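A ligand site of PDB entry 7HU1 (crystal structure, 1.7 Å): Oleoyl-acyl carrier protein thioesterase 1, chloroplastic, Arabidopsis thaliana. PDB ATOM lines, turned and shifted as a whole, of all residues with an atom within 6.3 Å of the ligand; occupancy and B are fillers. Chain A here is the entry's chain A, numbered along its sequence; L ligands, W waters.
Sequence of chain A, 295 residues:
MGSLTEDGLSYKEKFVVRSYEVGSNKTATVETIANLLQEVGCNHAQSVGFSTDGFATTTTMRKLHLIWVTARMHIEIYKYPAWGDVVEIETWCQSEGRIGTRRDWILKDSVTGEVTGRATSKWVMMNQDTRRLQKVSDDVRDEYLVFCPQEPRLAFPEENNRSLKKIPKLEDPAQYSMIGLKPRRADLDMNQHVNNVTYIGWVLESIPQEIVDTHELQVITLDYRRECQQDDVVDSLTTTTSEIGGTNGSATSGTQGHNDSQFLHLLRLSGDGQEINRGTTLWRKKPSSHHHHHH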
ATOM      1  N   GLN A  38     -12.212  32.902  -7.347  1.00  0.00           N
ATOM      2  CA  GLN A  38     -12.119  31.460  -7.098  1.00  0.00           C
ATOM      3  C   GLN A  38     -12.901  31.098  -5.830  1.00  0.00           C
ATOM      4  O   GLN A  38     -13.597  30.080  -5.808  1.00  0.00           O
ATOM      5  CB  GLN A  38     -10.639  31.034  -6.924  1.00  0.00           C
ATOM      6  CG  GLN A  38      -9.783  31.075  -8.197  1.00  0.00           C
ATOM      7  CD  GLN A  38      -8.618  30.084  -8.190  1.00  0.00           C
ATOM      8  OE1 GLN A  38      -8.222  29.556  -9.227  1.00  0.00           O
ATOM      9  NE2 GLN A  38      -8.045  29.821  -7.025  1.00  0.00           N
ATOM     10  N   GLY A  41     -16.616  31.265  -6.457  1.00  0.00           N
ATOM     11  CA  GLY A  41     -16.903  30.141  -7.352  1.00  0.00           C
ATOM     12  C   GLY A  41     -17.051  28.851  -6.564  1.00  0.00           C
ATOM     13  O   GLY A  41     -18.021  28.119  -6.763  1.00  0.00           O
ATOM     14  N   CYS A  42     -16.117  28.611  -5.650  1.00  0.00           N
ATOM     15  CA  CYS A  42     -16.110  27.446  -4.791  1.00  0.00           C
ATOM     16  C   CYS A  42     -17.352  27.403  -3.898  1.00  0.00           C
ATOM     17  O   CYS A  42     -17.973  26.350  -3.768  1.00  0.00           O
ATOM     18  CB  CYS A  42     -14.832  27.421  -3.962  1.00  0.00           C
ATOM     19  SG  CYS A  42     -14.622  25.920  -2.970  1.00  0.00           S
ATOM     20  N   ASN A  43     -17.746  28.551  -3.309  1.00  0.00           N
ATOM     21  CA  ASN A  43     -18.921  28.627  -2.458  1.00  0.00           C
ATOM     22  C   ASN A  43     -20.206  28.380  -3.254  1.00  0.00           C
ATOM     23  O   ASN A  43     -21.092  27.663  -2.783  1.00  0.00           O
ATOM     24  CB  ASN A  43     -18.949  29.928  -1.643  1.00  0.00           C
ATOM     25  CG  ASN A  43     -17.844  29.946  -0.597  1.00  0.00           C
ATOM     26  OD1 ASN A  43     -17.397  28.898  -0.124  1.00  0.00           O
ATOM     27  ND2 ASN A  43     -17.373  31.119  -0.232  1.00  0.00           N
ATOM     28  N   HIS A  44     -20.263  28.890  -4.485  1.00  0.00           N
ATOM     29  CA  HIS A  44     -21.414  28.644  -5.356  1.00  0.00           C
ATOM     30  C   HIS A  44     -21.550  27.126  -5.674  1.00  0.00           C
ATOM     31  O   HIS A  44     -22.631  26.572  -5.462  1.00  0.00           O
ATOM     32  CB  HIS A  44     -21.301  29.458  -6.664  1.00  0.00           C
ATOM     33  CG  HIS A  44     -22.475  29.271  -7.579  1.00  0.00           C
ATOM     34  ND1 HIS A  44     -22.360  29.433  -8.951  1.00  0.00           N
ATOM     35  CD2 HIS A  44     -23.759  28.913  -7.291  1.00  0.00           C
ATOM     36  CE1 HIS A  44     -23.572  29.235  -9.438  1.00  0.00           C
ATOM     37  NE2 HIS A  44     -24.432  28.883  -8.488  1.00  0.00           N
ATOM     38  N   ALA A  45     -20.454  26.458  -6.117  1.00  0.00           N
ATOM     39  CA  ALA A  45     -20.468  25.017  -6.426  1.00  0.00           C
ATOM     40  C   ALA A  45     -20.967  24.190  -5.210  1.00  0.00           C
ATOM     41  O   ALA A  45     -21.776  23.294  -5.387  1.00  0.00           O
ATOM     42  CB  ALA A  45     -19.084  24.550  -6.849  1.00  0.00           C
ATOM     43  N   VAL A  48     -24.773  24.507  -4.649  1.00  0.00           N
ATOM     44  CA  VAL A  48     -25.610  23.779  -5.610  1.00  0.00           C
ATOM     45  C   VAL A  48     -25.342  22.224  -5.623  1.00  0.00           C
ATOM     46  O   VAL A  48     -25.718  21.536  -6.570  1.00  0.00           O
ATOM     47  CB  VAL A  48     -25.577  24.398  -7.015  1.00  0.00           C
ATOM     48  CG1 VAL A  48     -26.070  25.853  -6.963  1.00  0.00           C
ATOM     49  CG2 VAL A  48     -24.174  24.346  -7.621  1.00  0.00           C
ATOM     50  N   PHE A  50     -22.334  20.261  -5.332  1.00  0.00           N
ATOM     51  CA  PHE A  50     -21.105  19.610  -5.827  1.00  0.00           C
ATOM     52  C   PHE A  50     -20.356  18.991  -4.641  1.00  0.00           C
ATOM     53  O   PHE A  50     -20.604  19.346  -3.487  1.00  0.00           O
ATOM     54  CB  PHE A  50     -20.195  20.608  -6.584  1.00  0.00           C
ATOM     55  CG  PHE A  50     -20.601  20.862  -8.016  1.00  0.00           C
ATOM     56  CD1 PHE A  50     -21.850  21.371  -8.323  1.00  0.00           C
ATOM     57  CD2 PHE A  50     -19.710  20.642  -9.044  1.00  0.00           C
ATOM     58  CE1 PHE A  50     -22.218  21.591  -9.641  1.00  0.00           C
ATOM     59  CE2 PHE A  50     -20.075  20.876 -10.363  1.00  0.00           C
ATOM     60  CZ  PHE A  50     -21.328  21.343 -10.656  1.00  0.00           C
ATOM     61  N   PHE A  55     -12.308  18.470  -5.303  1.00  0.00           N
ATOM     62  CA  PHE A  55     -12.292  18.449  -6.764  1.00  0.00           C
ATOM     63  C   PHE A  55     -13.551  18.940  -7.453  1.00  0.00           C
ATOM     64  O   PHE A  55     -13.594  18.908  -8.696  1.00  0.00           O
ATOM     65  CB  PHE A  55     -11.906  17.069  -7.296  1.00  0.00           C
ATOM     66  CG  PHE A  55     -10.410  16.935  -7.381  1.00  0.00           C
ATOM     67  CD1 PHE A  55      -9.679  17.659  -8.311  1.00  0.00           C
ATOM     68  CD2 PHE A  55      -9.716  16.150  -6.470  1.00  0.00           C
ATOM     69  CE1 PHE A  55      -8.295  17.551  -8.375  1.00  0.00           C
ATOM     70  CE2 PHE A  55      -8.336  16.043  -6.543  1.00  0.00           C
ATOM     71  CZ  PHE A  55      -7.632  16.742  -7.482  1.00  0.00           C
ATOM     72  N   ALA A  56     -14.555  19.416  -6.679  1.00  0.00           N
ATOM     73  CA  ALA A  56     -15.823  19.961  -7.197  1.00  0.00           C
ATOM     74  C   ALA A  56     -16.423  19.176  -8.371  1.00  0.00           C
ATOM     75  O   ALA A  56     -16.329  19.617  -9.520  1.00  0.00           O
ATOM     76  CB  ALA A  56     -15.643  21.426  -7.577  1.00  0.00           C
ATOM     77  N   TRP A  68     -13.145  19.139 -13.764  1.00  0.00           N
ATOM     78  CA  TRP A  68     -13.085  20.352 -14.577  1.00  0.00           C
ATOM     79  C   TRP A  68     -11.674  20.930 -14.469  1.00  0.00           C
ATOM     80  O   TRP A  68     -11.091  20.918 -13.385  1.00  0.00           O
ATOM     81  CB  TRP A  68     -14.092  21.406 -14.073  1.00  0.00           C
ATOM     82  CG  TRP A  68     -15.542  21.079 -14.314  1.00  0.00           C
ATOM     83  CD1 TRP A  68     -16.495  20.876 -13.373  1.00  0.00           C
ATOM     84  CD2 TRP A  68     -16.195  20.995 -15.576  1.00  0.00           C
ATOM     85  NE1 TRP A  68     -17.711  20.647 -13.968  1.00  0.00           N
ATOM     86  CE2 TRP A  68     -17.550  20.691 -15.331  1.00  0.00           C
ATOM     87  CE3 TRP A  68     -15.768  21.108 -16.910  1.00  0.00           C
ATOM     88  CZ2 TRP A  68     -18.474  20.520 -16.355  1.00  0.00           C
ATOM     89  CZ3 TRP A  68     -16.692  20.945 -17.922  1.00  0.00           C
ATOM     90  CH2 TRP A  68     -18.018  20.646 -17.635  1.00  0.00           C
ATOM     91  N   VAL A  69     -11.128  21.401 -15.579  1.00  0.00           N
ATOM     92  CA  VAL A  69      -9.852  22.099 -15.583  1.00  0.00           C
ATOM     93  C   VAL A  69     -10.043  23.437 -16.330  1.00  0.00           C
ATOM     94  O   VAL A  69     -10.844  23.501 -17.276  1.00  0.00           O
ATOM     95  CB  VAL A  69      -8.648  21.282 -16.123  1.00  0.00           C
ATOM     96  CG1 VAL A  69      -8.368  20.036 -15.274  1.00  0.00           C
ATOM     97  CG2 VAL A  69      -8.835  20.899 -17.579  1.00  0.00           C
ATOM     98  N   CYS A  93     -22.970  30.059 -13.619  1.00  0.00           N
ATOM     99  CA  CYS A  93     -22.403  29.184 -14.632  1.00  0.00           C
ATOM    100  C   CYS A  93     -23.364  28.986 -15.804  1.00  0.00           C
ATOM    101  O   CYS A  93     -24.571  29.157 -15.657  1.00  0.00           O
ATOM    102  CB  CYS A  93     -22.026  27.828 -14.040  1.00  0.00           C
ATOM    103  SG  CYS A  93     -20.698  27.906 -12.846  1.00  0.00           S
ATOM    104  N   THR A 101     -17.935  24.190 -19.974  1.00  0.00           N
ATOM    105  CA  THR A 101     -18.780  25.096 -19.204  1.00  0.00           C
ATOM    106  C   THR A 101     -18.078  26.450 -19.026  1.00  0.00           C
ATOM    107  O   THR A 101     -16.858  26.561 -19.231  1.00  0.00           O
ATOM    108  CB  THR A 101     -19.200  24.489 -17.858  1.00  0.00           C
ATOM    109  OG1 THR A 101     -18.034  24.101 -17.134  1.00  0.00           O
ATOM    110  CG2 THR A 101     -20.168  23.333 -18.007  1.00  0.00           C
ATOM    111  N   ARG A 102     -18.847  27.471 -18.647  1.00  0.00           N
ATOM    112  CA  ARG A 102     -18.348  28.812 -18.449  1.00  0.00           C
ATOM    113  C   ARG A 102     -18.796  29.316 -17.087  1.00  0.00           C
ATOM    114  O   ARG A 102     -19.941  29.057 -16.665  1.00  0.00           O
ATOM    115  CB  ARG A 102     -18.930  29.723 -19.546  1.00  0.00           C
ATOM    116  CG  ARG A 102     -18.210  31.064 -19.709  1.00  0.00           C
ATOM    117  CD  ARG A 102     -18.898  31.920 -20.778  1.00  0.00           C
ATOM    118  NE  ARG A 102     -20.044  32.624 -20.222  1.00  0.00           N
ATOM    119  CZ  ARG A 102     -21.318  32.310 -20.458  1.00  0.00           C
ATOM    120  NH1 ARG A 102     -22.288  32.980 -19.854  1.00  0.00           N
ATOM    121  NH2 ARG A 102     -21.625  31.339 -21.309  1.00  0.00           N
ATOM    122  N   ARG A 103     -17.902  30.025 -16.365  1.00  0.00           N
ATOM    123  CA  ARG A 103     -18.307  30.683 -15.133  1.00  0.00           C
ATOM    124  C   ARG A 103     -18.065  32.150 -15.354  1.00  0.00           C
ATOM    125  O   ARG A 103     -16.959  32.533 -15.790  1.00  0.00           O
ATOM    126  CB  ARG A 103     -17.539  30.210 -13.887  1.00  0.00           C
ATOM    127  CG  ARG A 103     -17.905  31.041 -12.649  1.00  0.00           C
ATOM    128  CD  ARG A 103     -17.304  30.508 -11.347  1.00  0.00           C
ATOM    129  NE  ARG A 103     -17.880  29.222 -10.964  1.00  0.00           N
ATOM    130  CZ  ARG A 103     -19.054  29.073 -10.360  1.00  0.00           C
ATOM    131  NH1 ARG A 103     -19.506  27.854 -10.057  1.00  0.00           N
ATOM    132  NH2 ARG A 103     -19.784  30.144 -10.043  1.00  0.00           N
ATOM    133  N   TRP A 105     -18.494  36.329 -13.705  1.00  0.00           N
ATOM    134  CA  TRP A 105     -18.537  37.118 -12.478  1.00  0.00           C
ATOM    135  C   TRP A 105     -18.746  38.608 -12.793  1.00  0.00           C
ATOM    136  O   TRP A 105     -18.293  39.091 -13.836  1.00  0.00           O
ATOM    137  CB  TRP A 105     -17.243  37.018 -11.645  1.00  0.00           C
ATOM    138  CG  TRP A 105     -16.752  35.669 -11.186  1.00  0.00           C
ATOM    139  CD1 TRP A 105     -16.782  35.190  -9.903  1.00  0.00           C
ATOM    140  CD2 TRP A 105     -15.930  34.756 -11.934  1.00  0.00           C
ATOM    141  NE1 TRP A 105     -16.106  33.991  -9.829  1.00  0.00           N
ATOM    142  CE2 TRP A 105     -15.531  33.720 -11.050  1.00  0.00           C
ATOM    143  CE3 TRP A 105     -15.466  34.723 -13.264  1.00  0.00           C
ATOM    144  CZ2 TRP A 105     -14.702  32.669 -11.458  1.00  0.00           C
ATOM    145  CZ3 TRP A 105     -14.649  33.662 -13.656  1.00  0.00           C
ATOM    146  CH2 TRP A 105     -14.288  32.649 -12.765  1.00  0.00           C
ATOM    147  N   SER A 121     -14.583  32.732 -17.390  1.00  0.00           N
ATOM    148  CA  SER A 121     -13.639  31.624 -17.444  1.00  0.00           C
ATOM    149  C   SER A 121     -14.264  30.470 -18.189  1.00  0.00           C
ATOM    150  O   SER A 121     -15.457  30.186 -17.987  1.00  0.00           O
ATOM    151  CB  SER A 121     -13.287  31.178 -16.021  1.00  0.00           C
ATOM    152  OG  SER A 121     -14.477  30.704 -15.424  1.00  0.00           O
ATOM    153  N   TRP A 123     -14.030  26.305 -18.791  1.00  0.00           N
ATOM    154  CA  TRP A 123     -13.608  25.059 -18.165  1.00  0.00           C
ATOM    155  C   TRP A 123     -13.864  23.892 -19.142  1.00  0.00           C
ATOM    156  O   TRP A 123     -14.845  23.905 -19.881  1.00  0.00           O
ATOM    157  CB  TRP A 123     -14.416  24.837 -16.861  1.00  0.00           C
ATOM    158  CG  TRP A 123     -14.212  25.912 -15.827  1.00  0.00           C
ATOM    159  CD1 TRP A 123     -14.805  27.139 -15.795  1.00  0.00           C
ATOM    160  CD2 TRP A 123     -13.310  25.870 -14.717  1.00  0.00           C
ATOM    161  NE1 TRP A 123     -14.346  27.850 -14.721  1.00  0.00           N
ATOM    162  CE2 TRP A 123     -13.445  27.088 -14.029  1.00  0.00           C
ATOM    163  CE3 TRP A 123     -12.426  24.905 -14.220  1.00  0.00           C
ATOM    164  CZ2 TRP A 123     -12.681  27.389 -12.906  1.00  0.00           C
ATOM    165  CZ3 TRP A 123     -11.721  25.178 -13.069  1.00  0.00           C
ATOM    166  CH2 TRP A 123     -11.877  26.391 -12.404  1.00  0.00           C
ATOM    167  N   TYR A 144     -26.447  20.377 -15.314  1.00  0.00           N
ATOM    168  CA  TYR A 144     -26.277  21.819 -15.335  1.00  0.00           C
ATOM    169  C   TYR A 144     -27.598  22.601 -15.537  1.00  0.00           C
ATOM    170  O   TYR A 144     -27.701  23.727 -15.053  1.00  0.00           O
ATOM    171  CB  TYR A 144     -25.195  22.234 -16.357  1.00  0.00           C
ATOM    172  CG  TYR A 144     -23.822  22.208 -15.717  1.00  0.00           C
ATOM    173  CD1 TYR A 144     -23.229  21.010 -15.349  1.00  0.00           C
ATOM    174  CD2 TYR A 144     -23.124  23.387 -15.472  1.00  0.00           C
ATOM    175  CE1 TYR A 144     -21.992  20.983 -14.722  1.00  0.00           C
ATOM    176  CE2 TYR A 144     -21.879  23.365 -14.849  1.00  0.00           C
ATOM    177  CZ  TYR A 144     -21.314  22.161 -14.467  1.00  0.00           C
ATOM    178  OH  TYR A 144     -20.113  22.079 -13.801  1.00  0.00           O
ATOM    179  N   PHE A 147     -29.122  24.216 -12.106  1.00  0.00           N
ATOM    180  CA  PHE A 147     -28.630  25.421 -11.430  1.00  0.00           C
ATOM    181  C   PHE A 147     -28.069  26.547 -12.328  1.00  0.00           C
ATOM    182  O   PHE A 147     -27.477  27.484 -11.803  1.00  0.00           O
ATOM    183  CB  PHE A 147     -27.571  25.035 -10.378  1.00  0.00           C
ATOM    184  CG  PHE A 147     -26.311  24.427 -10.965  1.00  0.00           C
ATOM    185  CD1 PHE A 147     -25.209  25.216 -11.262  1.00  0.00           C
ATOM    186  CD2 PHE A 147     -26.236  23.066 -11.216  1.00  0.00           C
ATOM    187  CE1 PHE A 147     -24.059  24.656 -11.818  1.00  0.00           C
ATOM    188  CE2 PHE A 147     -25.099  22.515 -11.788  1.00  0.00           C
ATOM    189  CZ  PHE A 147     -24.017  23.302 -12.075  1.00  0.00           C
HETATM  190  N1  LIG L   1     -14.850  25.440 -10.183  1.00  0.00           N
HETATM  191  N2  LIG L   1     -17.957  25.378 -11.181  1.00  0.00           N
HETATM  192  C1  LIG L   1     -13.792  23.301 -10.836  1.00  0.00           C
HETATM  193  C2  LIG L   1     -15.682  26.213 -10.907  1.00  0.00           C
HETATM  194  C3  LIG L   1     -16.754  25.540 -11.733  1.00  0.00           C
HETATM  195  C4  LIG L   1     -16.445  25.011 -12.984  1.00  0.00           C
HETATM  196  C5  LIG L   1     -17.497  24.399 -13.651  1.00  0.00           C
HETATM  197  C6  LIG L   1     -20.263  24.671 -11.306  1.00  0.00           C
HETATM  198  C7  LIG L   1     -14.348  26.543  -8.061  1.00  0.00           C
HETATM  199  C8  LIG L   1     -13.799  26.058  -9.371  1.00  0.00           C
HETATM  200  C9  LIG L   1     -14.949  23.983 -10.141  1.00  0.00           C
HETATM  201  C10 LIG L   1     -18.905  24.781 -11.910  1.00  0.00           C
HETATM  202  N3  LIG L   1     -18.724  24.267 -13.133  1.00  0.00           N
HETATM  203  O1  LIG L   1     -15.637  27.438 -10.904  1.00  0.00           O
HETATM  204  O   HOH W   1     -14.108  29.407  -9.839  1.00  0.00           O
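Gly 41 touches the ligand (C to C7, 3.9 Å). N of Cys 42 touches C7 of the ligand, at 3.6 Å. Phe 50 touches the ligand (CZ to C6, 3.6 Å). Ala 56 touches the ligand. Trp 68 touches the ligand. SG of Cys 93 touches C6 of the ligand, at 3.6 Å. Thr 101 touches the ligand (OG1 to C5, 3.5 Å). Trp 123 touches the ligand. Phe 147 touches the ligand. Hydrophobic or aromatic side chains within 4 Å of the ligand: Phe 50, Ala 56, Trp 68, Trp 123, Tyr 144 and Phe 147.
The side-chain hydroxyl (OH) of Tyr 144 sits at hydrogen-bond distance from the indole nitrogen (NE1) of Trp 68 (2.8 Å). The guanidinium group of Arg 103 lies within hydrogen-bond range of the side-chain sulfur of Cys 93 (3.0 Å). N of Ser 121 is in hydrogen-bond range of O of Arg 103. The guanidinium group of Arg 103 sits at hydrogen-bond distance from a ring nitrogen (ND1) of His 44 (2.9 Å). The backbone carbonyl oxygen (O) of Thr 101 is in hydrogen-bond range of the backbone NH (N) of Trp 123, 2.9 Å away. N of Phe 50 is in hydrogen-bond range of O of Ala 45, 3.1 Å away. The indole nitrogen (NE1) of Trp 123 sits at hydrogen-bond distance from the side-chain hydroxyl (OG) of Ser 121 (2.9 Å).
The side-chain hydroxyl (OH) of Tyr 144 lies within hydrogen-bond range of a nitrogen (N3) of the ligand (2.7 Å). An oxygen (O1) of the ligand sits at hydrogen-bond distance from the guanidinium group (NE) of Arg 103 (2.9 Å).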
